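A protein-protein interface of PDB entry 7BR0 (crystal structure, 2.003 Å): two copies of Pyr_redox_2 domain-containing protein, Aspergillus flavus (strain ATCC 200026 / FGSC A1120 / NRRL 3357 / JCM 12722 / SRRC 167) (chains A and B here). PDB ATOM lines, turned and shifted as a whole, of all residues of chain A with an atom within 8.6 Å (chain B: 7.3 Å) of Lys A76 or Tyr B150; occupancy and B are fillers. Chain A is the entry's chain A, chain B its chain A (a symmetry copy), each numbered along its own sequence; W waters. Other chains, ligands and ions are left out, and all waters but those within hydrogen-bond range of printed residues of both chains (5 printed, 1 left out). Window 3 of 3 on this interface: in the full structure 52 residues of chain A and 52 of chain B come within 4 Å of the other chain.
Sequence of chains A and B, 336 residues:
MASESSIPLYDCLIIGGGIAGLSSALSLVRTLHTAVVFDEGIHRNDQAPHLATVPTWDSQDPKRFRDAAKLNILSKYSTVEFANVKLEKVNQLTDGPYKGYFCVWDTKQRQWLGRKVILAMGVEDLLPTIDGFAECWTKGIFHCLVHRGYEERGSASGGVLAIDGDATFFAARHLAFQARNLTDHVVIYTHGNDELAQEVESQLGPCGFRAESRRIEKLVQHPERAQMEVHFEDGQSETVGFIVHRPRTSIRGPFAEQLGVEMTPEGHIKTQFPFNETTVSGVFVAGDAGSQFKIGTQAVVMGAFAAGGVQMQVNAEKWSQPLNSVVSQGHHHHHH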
ATOM      1  N   LEU A  26     -14.916  21.233  -0.218  1.00  0.00           N
ATOM      2  CA  LEU A  26     -16.321  21.474   0.097  1.00  0.00           C
ATOM      3  C   LEU A  26     -16.515  21.965   1.534  1.00  0.00           C
ATOM      4  O   LEU A  26     -17.446  22.719   1.818  1.00  0.00           O
ATOM      5  CB  LEU A  26     -17.140  20.202  -0.129  1.00  0.00           C
ATOM      6  CG  LEU A  26     -18.649  20.322   0.098  1.00  0.00           C
ATOM      7  CD1 LEU A  26     -19.264  21.343  -0.851  1.00  0.00           C
ATOM      8  CD2 LEU A  26     -19.325  18.970  -0.064  1.00  0.00           C
ATOM      9  N   SER A  27     -15.647  21.531   2.443  1.00  0.00           N
ATOM     10  CA  SER A  27     -15.694  22.025   3.819  1.00  0.00           C
ATOM     11  C   SER A  27     -15.060  23.414   3.929  1.00  0.00           C
ATOM     12  O   SER A  27     -15.544  24.265   4.677  1.00  0.00           O
ATOM     13  CB  SER A  27     -14.992  21.051   4.772  1.00  0.00           C
ATOM     14  OG  SER A  27     -15.830  19.949   5.092  1.00  0.00           O
ATOM     15  N   LEU A  28     -13.982  23.643   3.182  1.00  0.00           N
ATOM     16  CA  LEU A  28     -13.263  24.917   3.253  1.00  0.00           C
ATOM     17  C   LEU A  28     -14.067  26.099   2.700  1.00  0.00           C
ATOM     18  O   LEU A  28     -13.919  27.226   3.178  1.00  0.00           O
ATOM     19  CB  LEU A  28     -11.925  24.821   2.507  1.00  0.00           C
ATOM     20  CG  LEU A  28     -10.819  23.968   3.149  1.00  0.00           C
ATOM     21  CD1 LEU A  28      -9.570  23.969   2.282  1.00  0.00           C
ATOM     22  CD2 LEU A  28     -10.477  24.455   4.553  1.00  0.00           C
ATOM     23  N   VAL A  29     -14.910  25.863   1.696  1.00  0.00           N
ATOM     24  CA  VAL A  29     -15.691  26.961   1.121  1.00  0.00           C
ATOM     25  C   VAL A  29     -16.733  27.465   2.120  1.00  0.00           C
ATOM     26  O   VAL A  29     -17.104  28.640   2.098  1.00  0.00           O
ATOM     27  CB  VAL A  29     -16.408  26.564  -0.191  1.00  0.00           C
ATOM     28  CG1 VAL A  29     -15.407  26.384  -1.316  1.00  0.00           C
ATOM     29  CG2 VAL A  29     -17.263  25.308  -0.004  1.00  0.00           C
ATOM     30  N   ARG A  30     -17.194  26.578   2.998  1.00  0.00           N
ATOM     31  CA  ARG A  30     -18.207  26.934   3.990  1.00  0.00           C
ATOM     32  C   ARG A  30     -17.689  27.940   5.017  1.00  0.00           C
ATOM     33  O   ARG A  30     -18.476  28.621   5.675  1.00  0.00           O
ATOM     34  CB  ARG A  30     -18.709  25.677   4.712  1.00  0.00           C
ATOM     35  CG  ARG A  30     -19.514  24.722   3.834  1.00  0.00           C
ATOM     36  CD  ARG A  30     -20.815  25.360   3.356  1.00  0.00           C
ATOM     37  NE  ARG A  30     -21.640  25.821   4.472  1.00  0.00           N
ATOM     38  CZ  ARG A  30     -22.733  26.568   4.337  1.00  0.00           C
ATOM     39  NH1 ARG A  30     -23.139  26.951   3.133  1.00  0.00           N
ATOM     40  NH2 ARG A  30     -23.418  26.941   5.411  1.00  0.00           N
ATOM     41  N   THR A  31     -16.368  28.018   5.154  1.00  0.00           N
ATOM     42  CA  THR A  31     -15.740  28.897   6.134  1.00  0.00           C
ATOM     43  C   THR A  31     -14.932  30.011   5.453  1.00  0.00           C
ATOM     44  O   THR A  31     -14.136  30.694   6.100  1.00  0.00           O
ATOM     45  CB  THR A  31     -14.836  28.091   7.093  1.00  0.00           C
ATOM     46  OG1 THR A  31     -13.936  27.266   6.342  1.00  0.00           O
ATOM     47  CG2 THR A  31     -15.686  27.198   7.996  1.00  0.00           C
ATOM     48  N   LEU A  32     -15.166  30.188   4.153  1.00  0.00           N
ATOM     49  CA  LEU A  32     -14.533  31.236   3.342  1.00  0.00           C
ATOM     50  C   LEU A  32     -13.012  31.099   3.219  1.00  0.00           C
ATOM     51  O   LEU A  32     -12.332  32.024   2.767  1.00  0.00           O
ATOM     52  CB  LEU A  32     -14.877  32.626   3.899  1.00  0.00           C
ATOM     53  CG  LEU A  32     -16.342  33.046   3.772  1.00  0.00           C
ATOM     54  CD1 LEU A  32     -16.599  34.315   4.558  1.00  0.00           C
ATOM     55  CD2 LEU A  32     -16.712  33.247   2.315  1.00  0.00           C
ATOM     56  N   HIS A  33     -12.472  29.945   3.589  1.00  0.00           N
ATOM     57  CA  HIS A  33     -11.042  29.721   3.431  1.00  0.00           C
ATOM     58  C   HIS A  33     -10.712  29.526   1.956  1.00  0.00           C
ATOM     59  O   HIS A  33     -11.536  29.028   1.182  1.00  0.00           O
ATOM     60  CB  HIS A  33     -10.582  28.523   4.264  1.00  0.00           C
ATOM     61  CG  HIS A  33     -10.602  28.782   5.740  1.00  0.00           C
ATOM     62  ND1 HIS A  33     -11.645  28.392   6.551  1.00  0.00           N
ATOM     63  CD2 HIS A  33      -9.717  29.421   6.543  1.00  0.00           C
ATOM     64  CE1 HIS A  33     -11.395  28.765   7.795  1.00  0.00           C
ATOM     65  NE2 HIS A  33     -10.232  29.391   7.817  1.00  0.00           N
ATOM     66  N   LYS A  70     -17.779  19.089  -8.001  1.00  0.00           N
ATOM     67  CA  LYS A  70     -17.059  20.307  -8.365  1.00  0.00           C
ATOM     68  C   LYS A  70     -18.021  21.432  -8.745  1.00  0.00           C
ATOM     69  O   LYS A  70     -17.834  22.582  -8.345  1.00  0.00           O
ATOM     70  CB  LYS A  70     -16.097  20.025  -9.520  1.00  0.00           C
ATOM     71  CG  LYS A  70     -15.340  21.240 -10.026  1.00  0.00           C
ATOM     72  CD  LYS A  70     -14.391  20.868 -11.155  1.00  0.00           C
ATOM     73  CE  LYS A  70     -13.745  22.101 -11.769  1.00  0.00           C
ATOM     74  NZ  LYS A  70     -12.803  21.754 -12.876  1.00  0.00           N
ATOM     75  N   LEU A  71     -19.044  21.101  -9.528  1.00  0.00           N
ATOM     76  CA  LEU A  71     -20.032  22.091  -9.948  1.00  0.00           C
ATOM     77  C   LEU A  71     -20.821  22.576  -8.738  1.00  0.00           C
ATOM     78  O   LEU A  71     -21.117  23.764  -8.599  1.00  0.00           O
ATOM     79  CB  LEU A  71     -20.976  21.497 -10.998  1.00  0.00           C
ATOM     80  CG  LEU A  71     -22.052  22.431 -11.563  1.00  0.00           C
ATOM     81  CD1 LEU A  71     -21.424  23.565 -12.362  1.00  0.00           C
ATOM     82  CD2 LEU A  71     -23.040  21.654 -12.420  1.00  0.00           C
ATOM     83  N   ASN A  72     -21.152  21.632  -7.866  1.00  0.00           N
ATOM     84  CA  ASN A  72     -21.867  21.916  -6.630  1.00  0.00           C
ATOM     85  C   ASN A  72     -21.076  22.876  -5.739  1.00  0.00           C
ATOM     86  O   ASN A  72     -21.648  23.540  -4.873  1.00  0.00           O
ATOM     87  CB  ASN A  72     -22.159  20.600  -5.901  1.00  0.00           C
ATOM     88  CG  ASN A  72     -22.905  20.794  -4.599  1.00  0.00           C
ATOM     89  OD1 ASN A  72     -23.877  21.552  -4.519  1.00  0.00           O
ATOM     90  ND2 ASN A  72     -22.452  20.097  -3.562  1.00  0.00           N
ATOM     91  N   ILE A  73     -19.762  22.942  -5.963  1.00  0.00           N
ATOM     92  CA  ILE A  73     -18.900  23.909  -5.285  1.00  0.00           C
ATOM     93  C   ILE A  73     -18.867  25.232  -6.047  1.00  0.00           C
ATOM     94  O   ILE A  73     -19.180  26.287  -5.490  1.00  0.00           O
ATOM     95  CB  ILE A  73     -17.444  23.381  -5.131  1.00  0.00           C
ATOM     96  CG1 ILE A  73     -17.388  22.251  -4.099  1.00  0.00           C
ATOM     97  CG2 ILE A  73     -16.488  24.502  -4.699  1.00  0.00           C
ATOM     98  CD1 ILE A  73     -16.036  21.547  -4.011  1.00  0.00           C
ATOM     99  N   LEU A  74     -18.480  25.172  -7.320  1.00  0.00           N
ATOM    100  CA  LEU A  74     -18.234  26.382  -8.104  1.00  0.00           C
ATOM    101  C   LEU A  74     -19.508  27.170  -8.418  1.00  0.00           C
ATOM    102  O   LEU A  74     -19.441  28.342  -8.782  1.00  0.00           O
ATOM    103  CB  LEU A  74     -17.521  26.026  -9.412  1.00  0.00           C
ATOM    104  CG  LEU A  74     -16.093  25.486  -9.293  1.00  0.00           C
ATOM    105  CD1 LEU A  74     -15.532  25.144 -10.671  1.00  0.00           C
ATOM    106  CD2 LEU A  74     -15.180  26.487  -8.581  1.00  0.00           C
ATOM    107  N   SER A  75     -20.667  26.535  -8.278  1.00  0.00           N
ATOM    108  CA  SER A  75     -21.924  27.208  -8.591  1.00  0.00           C
ATOM    109  C   SER A  75     -22.332  28.206  -7.507  1.00  0.00           C
ATOM    110  O   SER A  75     -23.179  29.066  -7.749  1.00  0.00           O
ATOM    111  CB  SER A  75     -23.045  26.189  -8.790  1.00  0.00           C
ATOM    112  OG  SER A  75     -23.383  25.563  -7.567  1.00  0.00           O
ATOM    113  N   LYS A  76     -21.736  28.092  -6.321  1.00  0.00           N
ATOM    114  CA  LYS A  76     -22.119  28.939  -5.189  1.00  0.00           C
ATOM    115  C   LYS A  76     -20.930  29.655  -4.539  1.00  0.00           C
ATOM    116  O   LYS A  76     -21.062  30.788  -4.090  1.00  0.00           O
ATOM    117  CB  LYS A  76     -22.856  28.101  -4.138  1.00  0.00           C
ATOM    118  CG  LYS A  76     -23.186  28.865  -2.857  1.00  0.00           C
ATOM    119  CD  LYS A  76     -24.182  28.114  -1.992  1.00  0.00           C
ATOM    120  CE  LYS A  76     -24.423  28.841  -0.676  1.00  0.00           C
ATOM    121  NZ  LYS A  76     -25.509  28.205   0.126  1.00  0.00           N
ATOM    122  N   TYR A  77     -19.776  28.998  -4.497  1.00  0.00           N
ATOM    123  CA  TYR A  77     -18.621  29.518  -3.765  1.00  0.00           C
ATOM    124  C   TYR A  77     -17.522  29.985  -4.712  1.00  0.00           C
ATOM    125  O   TYR A  77     -17.459  29.535  -5.856  1.00  0.00           O
ATOM    126  CB  TYR A  77     -18.091  28.444  -2.815  1.00  0.00           C
ATOM    127  CG  TYR A  77     -19.171  27.856  -1.940  1.00  0.00           C
ATOM    128  CD1 TYR A  77     -19.552  28.482  -0.761  1.00  0.00           C
ATOM    129  CD2 TYR A  77     -19.817  26.679  -2.298  1.00  0.00           C
ATOM    130  CE1 TYR A  77     -20.541  27.953   0.042  1.00  0.00           C
ATOM    131  CE2 TYR A  77     -20.810  26.138  -1.502  1.00  0.00           C
ATOM    132  CZ  TYR A  77     -21.170  26.780  -0.333  1.00  0.00           C
ATOM    133  OH  TYR A  77     -22.158  26.251   0.467  1.00  0.00           O
ATOM    134  N   SER A  78     -16.657  30.883  -4.233  1.00  0.00           N
ATOM    135  CA  SER A  78     -15.610  31.458  -5.079  1.00  0.00           C
ATOM    136  C   SER A  78     -14.229  31.572  -4.422  1.00  0.00           C
ATOM    137  O   SER A  78     -13.363  32.283  -4.934  1.00  0.00           O
ATOM    138  CB  SER A  78     -16.052  32.844  -5.554  1.00  0.00           C
ATOM    139  OG  SER A  78     -16.275  33.707  -4.455  1.00  0.00           O
ATOM    140  N   THR A  79     -14.011  30.877  -3.306  1.00  0.00           N
ATOM    141  CA  THR A  79     -12.718  30.947  -2.623  1.00  0.00           C
ATOM    142  C   THR A  79     -11.816  29.752  -2.957  1.00  0.00           C
ATOM    143  O   THR A  79     -10.638  29.747  -2.600  1.00  0.00           O
ATOM    144  CB  THR A  79     -12.887  31.031  -1.088  1.00  0.00           C
ATOM    145  OG1 THR A  79     -13.499  29.832  -0.594  1.00  0.00           O
ATOM    146  CG2 THR A  79     -13.739  32.249  -0.708  1.00  0.00           C
ATOM    147  N   HIS B  50     -30.666  23.072   5.050  1.00  0.00           N
ATOM    148  CA  HIS B  50     -29.880  22.356   4.055  1.00  0.00           C
ATOM    149  C   HIS B  50     -28.865  21.415   4.696  1.00  0.00           C
ATOM    150  O   HIS B  50     -28.729  21.363   5.918  1.00  0.00           O
ATOM    151  CB  HIS B  50     -29.161  23.341   3.126  1.00  0.00           C
ATOM    152  CG  HIS B  50     -28.203  24.254   3.828  1.00  0.00           C
ATOM    153  ND1 HIS B  50     -27.061  23.801   4.453  1.00  0.00           N
ATOM    154  CD2 HIS B  50     -28.212  25.600   3.992  1.00  0.00           C
ATOM    155  CE1 HIS B  50     -26.411  24.826   4.975  1.00  0.00           C
ATOM    156  NE2 HIS B  50     -27.087  25.928   4.709  1.00  0.00           N
ATOM    157  N   ASP B  58     -24.472  19.764  -1.085  1.00  0.00           N
ATOM    158  CA  ASP B  58     -24.355  21.058  -0.419  1.00  0.00           C
ATOM    159  C   ASP B  58     -25.503  21.990  -0.791  1.00  0.00           C
ATOM    160  O   ASP B  58     -25.888  22.082  -1.958  1.00  0.00           O
ATOM    161  CB  ASP B  58     -23.027  21.732  -0.760  1.00  0.00           C
ATOM    162  CG  ASP B  58     -22.882  23.088  -0.098  1.00  0.00           C
ATOM    163  OD1 ASP B  58     -22.440  23.132   1.068  1.00  0.00           O
ATOM    164  OD2 ASP B  58     -23.217  24.110  -0.738  1.00  0.00           O
ATOM    165  N   SER B  59     -26.039  22.670   0.221  1.00  0.00           N
ATOM    166  CA  SER B  59     -27.120  23.648   0.062  1.00  0.00           C
ATOM    167  C   SER B  59     -28.425  23.010  -0.425  1.00  0.00           C
ATOM    168  O   SER B  59     -29.343  23.715  -0.853  1.00  0.00           O
ATOM    169  CB  SER B  59     -26.693  24.772  -0.896  1.00  0.00           C
ATOM    170  OG  SER B  59     -25.592  25.497  -0.372  1.00  0.00           O
ATOM    171  N   GLN B  60     -28.505  21.683  -0.339  1.00  0.00           N
ATOM    172  CA  GLN B  60     -29.718  20.944  -0.688  1.00  0.00           C
ATOM    173  C   GLN B  60     -30.443  20.497   0.576  1.00  0.00           C
ATOM    174  O   GLN B  60     -29.845  20.425   1.647  1.00  0.00           O
ATOM    175  CB  GLN B  60     -29.380  19.729  -1.557  1.00  0.00           C
ATOM    176  CG  GLN B  60     -28.551  20.060  -2.787  1.00  0.00           C
ATOM    177  CD  GLN B  60     -29.170  21.161  -3.624  1.00  0.00           C
ATOM    178  OE1 GLN B  60     -30.370  21.147  -3.898  1.00  0.00           O
ATOM    179  NE2 GLN B  60     -28.353  22.127  -4.029  1.00  0.00           N
ATOM    180  N   PHE B 142     -26.806  28.424  15.601  1.00  0.00           N
ATOM    181  CA  PHE B 142     -26.220  27.314  14.855  1.00  0.00           C
ATOM    182  C   PHE B 142     -25.343  26.448  15.748  1.00  0.00           C
ATOM    183  O   PHE B 142     -24.675  26.950  16.650  1.00  0.00           O
ATOM    184  CB  PHE B 142     -25.382  27.838  13.686  1.00  0.00           C
ATOM    185  CG  PHE B 142     -26.090  28.842  12.825  1.00  0.00           C
ATOM    186  CD1 PHE B 142     -27.444  28.728  12.566  1.00  0.00           C
ATOM    187  CD2 PHE B 142     -25.394  29.904  12.269  1.00  0.00           C
ATOM    188  CE1 PHE B 142     -28.093  29.655  11.769  1.00  0.00           C
ATOM    189  CE2 PHE B 142     -26.037  30.832  11.473  1.00  0.00           C
ATOM    190  CZ  PHE B 142     -27.388  30.705  11.221  1.00  0.00           C
ATOM    191  N   LEU B 145     -20.430  26.037  12.684  1.00  0.00           N
ATOM    192  CA  LEU B 145     -20.280  27.116  11.711  1.00  0.00           C
ATOM    193  C   LEU B 145     -19.696  26.629  10.381  1.00  0.00           C
ATOM    194  O   LEU B 145     -19.462  27.428   9.476  1.00  0.00           O
ATOM    195  CB  LEU B 145     -19.429  28.253  12.294  1.00  0.00           C
ATOM    196  CG  LEU B 145     -20.141  29.115  13.354  1.00  0.00           C
ATOM    197  CD1 LEU B 145     -19.199  30.168  13.946  1.00  0.00           C
ATOM    198  CD2 LEU B 145     -21.392  29.800  12.794  1.00  0.00           C
ATOM    199  N   VAL B 146     -19.480  25.319  10.255  1.00  0.00           N
ATOM    200  CA  VAL B 146     -19.191  24.720   8.953  1.00  0.00           C
ATOM    201  C   VAL B 146     -20.516  24.404   8.258  1.00  0.00           C
ATOM    202  O   VAL B 146     -20.644  24.536   7.039  1.00  0.00           O
ATOM    203  CB  VAL B 146     -18.342  23.429   9.069  1.00  0.00           C
ATOM    204  CG1 VAL B 146     -18.071  22.828   7.688  1.00  0.00           C
ATOM    205  CG2 VAL B 146     -17.027  23.712   9.783  1.00  0.00           C
ATOM    206  N   HIS B 147     -21.503  23.997   9.051  1.00  0.00           N
ATOM    207  CA  HIS B 147     -22.797  23.571   8.520  1.00  0.00           C
ATOM    208  C   HIS B 147     -23.743  24.750   8.298  1.00  0.00           C
ATOM    209  O   HIS B 147     -24.636  24.683   7.460  1.00  0.00           O
ATOM    210  CB  HIS B 147     -23.439  22.553   9.463  1.00  0.00           C
ATOM    211  CG  HIS B 147     -22.592  21.342   9.704  1.00  0.00           C
ATOM    212  ND1 HIS B 147     -22.922  20.371  10.626  1.00  0.00           N
ATOM    213  CD2 HIS B 147     -21.428  20.943   9.140  1.00  0.00           C
ATOM    214  CE1 HIS B 147     -21.998  19.428  10.619  1.00  0.00           C
ATOM    215  NE2 HIS B 147     -21.079  19.751   9.727  1.00  0.00           N
ATOM    216  N   ARG B 148     -23.539  25.821   9.059  1.00  0.00           N
ATOM    217  CA  ARG B 148     -24.323  27.049   8.923  1.00  0.00           C
ATOM    218  C   ARG B 148     -23.391  28.244   9.088  1.00  0.00           C
ATOM    219  O   ARG B 148     -22.315  28.107   9.656  1.00  0.00           O
ATOM    220  CB  ARG B 148     -25.446  27.108   9.966  1.00  0.00           C
ATOM    221  CG  ARG B 148     -26.510  26.021   9.841  1.00  0.00           C
ATOM    222  CD  ARG B 148     -27.357  26.189   8.588  1.00  0.00           C
ATOM    223  NE  ARG B 148     -28.155  27.413   8.612  1.00  0.00           N
ATOM    224  CZ  ARG B 148     -29.307  27.549   9.264  1.00  0.00           C
ATOM    225  NH1 ARG B 148     -29.808  26.543   9.969  1.00  0.00           N
ATOM    226  NH2 ARG B 148     -29.961  28.701   9.219  1.00  0.00           N
ATOM    227  N   GLY B 149     -23.800  29.409   8.592  1.00  0.00           N
ATOM    228  CA  GLY B 149     -23.064  30.640   8.832  1.00  0.00           C
ATOM    229  C   GLY B 149     -22.630  31.357   7.567  1.00  0.00           C
ATOM    230  O   GLY B 149     -22.674  32.582   7.508  1.00  0.00           O
ATOM    231  N   TYR B 150     -22.207  30.598   6.560  1.00  0.00           N
ATOM    232  CA  TYR B 150     -21.790  31.189   5.288  1.00  0.00           C
ATOM    233  C   TYR B 150     -22.840  32.166   4.768  1.00  0.00           C
ATOM    234  O   TYR B 150     -22.510  33.247   4.291  1.00  0.00           O
ATOM    235  CB  TYR B 150     -21.539  30.102   4.242  1.00  0.00           C
ATOM    236  CG  TYR B 150     -21.171  30.658   2.885  1.00  0.00           C
ATOM    237  CD1 TYR B 150     -19.853  30.965   2.574  1.00  0.00           C
ATOM    238  CD2 TYR B 150     -22.144  30.890   1.918  1.00  0.00           C
ATOM    239  CE1 TYR B 150     -19.510  31.478   1.339  1.00  0.00           C
ATOM    240  CE2 TYR B 150     -21.810  31.403   0.677  1.00  0.00           C
ATOM    241  CZ  TYR B 150     -20.491  31.695   0.396  1.00  0.00           C
ATOM    242  OH  TYR B 150     -20.149  32.207  -0.833  1.00  0.00           O
ATOM    243  N   GLU B 151     -24.105  31.778   4.874  1.00  0.00           N
ATOM    244  CA  GLU B 151     -25.202  32.596   4.374  1.00  0.00           C
ATOM    245  C   GLU B 151     -25.366  33.888   5.186  1.00  0.00           C
ATOM    246  O   GLU B 151     -26.033  34.824   4.744  1.00  0.00           O
ATOM    247  CB  GLU B 151     -26.508  31.793   4.386  1.00  0.00           C
ATOM    248  CG  GLU B 151     -26.561  30.654   3.357  1.00  0.00           C
ATOM    249  CD  GLU B 151     -25.629  29.487   3.682  1.00  0.00           C
ATOM    250  OE1 GLU B 151     -25.302  29.279   4.871  1.00  0.00           O
ATOM    251  OE2 GLU B 151     -25.222  28.776   2.739  1.00  0.00           O
ATOM    252  N   GLU B 152     -24.744  33.930   6.363  1.00  0.00           N
ATOM    253  CA  GLU B 152     -24.804  35.096   7.244  1.00  0.00           C
ATOM    254  C   GLU B 152     -23.526  35.937   7.183  1.00  0.00           C
ATOM    255  O   GLU B 152     -23.337  36.847   7.991  1.00  0.00           O
ATOM    256  CB  GLU B 152     -25.055  34.654   8.689  1.00  0.00           C
ATOM    257  CG  GLU B 152     -26.466  34.161   8.958  1.00  0.00           C
ATOM    258  CD  GLU B 152     -26.788  32.859   8.255  1.00  0.00           C
ATOM    259  OE1 GLU B 152     -25.968  31.919   8.324  1.00  0.00           O
ATOM    260  OE2 GLU B 152     -27.866  32.779   7.626  1.00  0.00           O
ATOM    261  N   ARG B 153     -22.649  35.637   6.231  1.00  0.00           N
ATOM    262  CA  ARG B 153     -21.413  36.397   6.092  1.00  0.00           C
ATOM    263  C   ARG B 153     -21.747  37.863   5.834  1.00  0.00           C
ATOM    264  O   ARG B 153     -22.702  38.170   5.131  1.00  0.00           O
ATOM    265  CB  ARG B 153     -20.544  35.829   4.966  1.00  0.00           C
ATOM    266  CG  ARG B 153     -21.116  36.029   3.573  1.00  0.00           C
ATOM    267  CD  ARG B 153     -20.443  35.100   2.567  1.00  0.00           C
ATOM    268  NE  ARG B 153     -20.896  35.332   1.197  1.00  0.00           N
ATOM    269  CZ  ARG B 153     -22.109  35.021   0.744  1.00  0.00           C
ATOM    270  NH1 ARG B 153     -23.007  34.464   1.548  1.00  0.00           N
ATOM    271  NH2 ARG B 153     -22.425  35.271  -0.517  1.00  0.00           N
ATOM    272  N   GLY B 154     -20.975  38.763   6.433  1.00  0.00           N
ATOM    273  CA  GLY B 154     -21.203  40.187   6.280  1.00  0.00           C
ATOM    274  C   GLY B 154     -22.185  40.752   7.290  1.00  0.00           C
ATOM    275  O   GLY B 154     -22.501  41.942   7.246  1.00  0.00           O
ATOM    276  N   LEU B 182     -16.928  35.506   9.445  1.00  0.00           N
ATOM    277  CA  LEU B 182     -18.249  35.870   8.927  1.00  0.00           C
ATOM    278  C   LEU B 182     -18.668  37.306   9.263  1.00  0.00           C
ATOM    279  O   LEU B 182     -19.607  37.834   8.668  1.00  0.00           O
ATOM    280  CB  LEU B 182     -19.309  34.913   9.477  1.00  0.00           C
ATOM    281  CG  LEU B 182     -19.146  33.420   9.178  1.00  0.00           C
ATOM    282  CD1 LEU B 182     -20.228  32.633   9.897  1.00  0.00           C
ATOM    283  CD2 LEU B 182     -19.193  33.138   7.686  1.00  0.00           C
HETATM  284  O   HOH W   1     -20.500  21.967   2.347  1.00  0.00           O
HETATM  285  O   HOH W   2     -22.168  32.580  -2.609  1.00  0.00           O
HETATM  286  O   HOH W   3     -23.803  24.455  -3.421  1.00  0.00           O
HETATM  287  O   HOH W   4     -18.421  29.662   8.468  1.00  0.00           O
HETATM  288  O   HOH W   5     -17.391  32.043  -1.601  1.00  0.00           O
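Among the printed residues, merely in contact across the chains: Leu A26 with Asp B58 (3.8 Å), Val A29 with Tyr B150 (3.6 Å), Arg A30 with His B50 (3.7 Å), Arg A30 with Asp B58 (3.6 Å), Arg A30 with Arg B148 (3.6 Å), Arg A30 with Tyr B150 (3.7 Å), Leu A32 with Tyr B150 (3.5 Å), Lys A76 with Tyr B150 (3.7 Å), Tyr A77 with Ser B59 (3.6 Å) and Tyr A77 with Tyr B150 (3.5 Å).
Of the printed residues of chain B, Tyr A77 touches Asp B58, Ser B59 and Tyr B150.
Ser A78 touches none of the printed residues of chain B.
Of the printed residues of chain A, His B50 touches Arg A30 (3.7 Å).
Leu B145 touches none of the printed residues of chain A.
Of the printed residues of chain A, Val B146 touches Arg A30.
Of the printed residues of chain A, His B147 touches Arg A30.
Of the printed residues of chain A, Arg B148 touches Arg A30 (3.6 Å).
No residue of chain A comes within 4 Å of Gly B149.
Of the printed residues of chain A, Tyr B150 touches Val A29, Arg A30, Leu A32, Lys A76 and Tyr A77.
Glu B151 touches just these residues of chain A: Arg A30 (2.8 Å) and Lys A76 (2.7 Å).
The nearest residue of chain B that does not touch Lys A76 is Asp B58 (4.3 Å).
The nearest residue of chain A that does not touch Tyr B150 is Ser A78 (5.1 Å).
The side-chain hydroxyl of Tyr A77 sits at hydrogen-bond distance from the guanidinium group of Arg A30, at 2.9 Å.
OG of Ser B59 is in hydrogen-bond range of OD2 of Asp B58 (2.8 Å).
The backbone carbonyl oxygen (O) of Asp B58 is in hydrogen-bond range of the side-chain amide nitrogen (NE2) of Gln B60.
O of Tyr B150 is in hydrogen-bond range of NH1 of Arg B153.
Printed residues of chain A that touch a printed residue of chain B: Leu A26, Val A29, Arg A30, Leu A32, Asn A72, Lys A76 and Tyr A77.
Hydrophobic or aromatic side chains of chain A within 4 Å of the printed part of chain B: Leu A26, Leu A32 and Tyr A77.
Printed residues of chain B that touch a printed residue of chain A: His B50, Asp B58, Ser B59, Val B146, His B147, Arg B148, Tyr B150 and Glu B151.
Hydrophobic or aromatic side chains of chain B that line the printed part of chain A: His B50 and Tyr B150.
Along chain B the printed residues that touch a printed residue of chain A span positions 50 to 151.
Among the printed residues, Asp or Glu carboxylates within 4 Å of a Lys or Arg side-chain nitrogen of the other chain: Arg A30 with Glu B151 and Lys A76 with Glu B151.
Water W1 lies within hydrogen-bond range of OD1 of Asp B58 and O of Leu A26.
Water W4 bridges the backbone carbonyl oxygen of Leu B145 (2.7 Å) and the backbone carbonyl oxygen of Arg A30 (3.0 Å).
Water W3 bridges the backbone carbonyl oxygen of Asn A72 (2.8 Å) and the side-chain carboxylate of Asp B58 (2.8 Å).
Water W5 lies within hydrogen-bond range of OH of Tyr B150 and N of Ser A78.
The guanidinium group (NE) of Arg A30 sits at hydrogen-bond distance from the backbone carbonyl oxygen (O) of Val B146 (3.0 Å).
The guanidinium group of Arg A30 lies within hydrogen-bond range of the backbone carbonyl oxygen of His B147 (3.3 Å).
The side-chain carboxylate of Glu B151 lies within salt-bridge range of the guanidinium group of Arg A30.
The backbone NH (N) of Asp B58 lies close to the side-chain amide nitrogen (ND2) of Asn A72 (3.2 Å).
The side-chain amino group (NZ) of Lys A76 sits at hydrogen-bond distance from the side-chain hydroxyl (OG) of Ser B59 (2.8 Å).
The side-chain amino group (NZ) of Lys A76 lies within salt-bridge range of the side-chain carboxylate (OE2) of Glu B151, at 2.7 Å.
OH of Tyr A77 sits at hydrogen-bond distance from OD2 of Asp B58 (2.7 Å).
No position is printed for both chains.
Of the 17 pairs that touch across the chains among the printed residues, none has its exchanged pair printed and touching as well.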
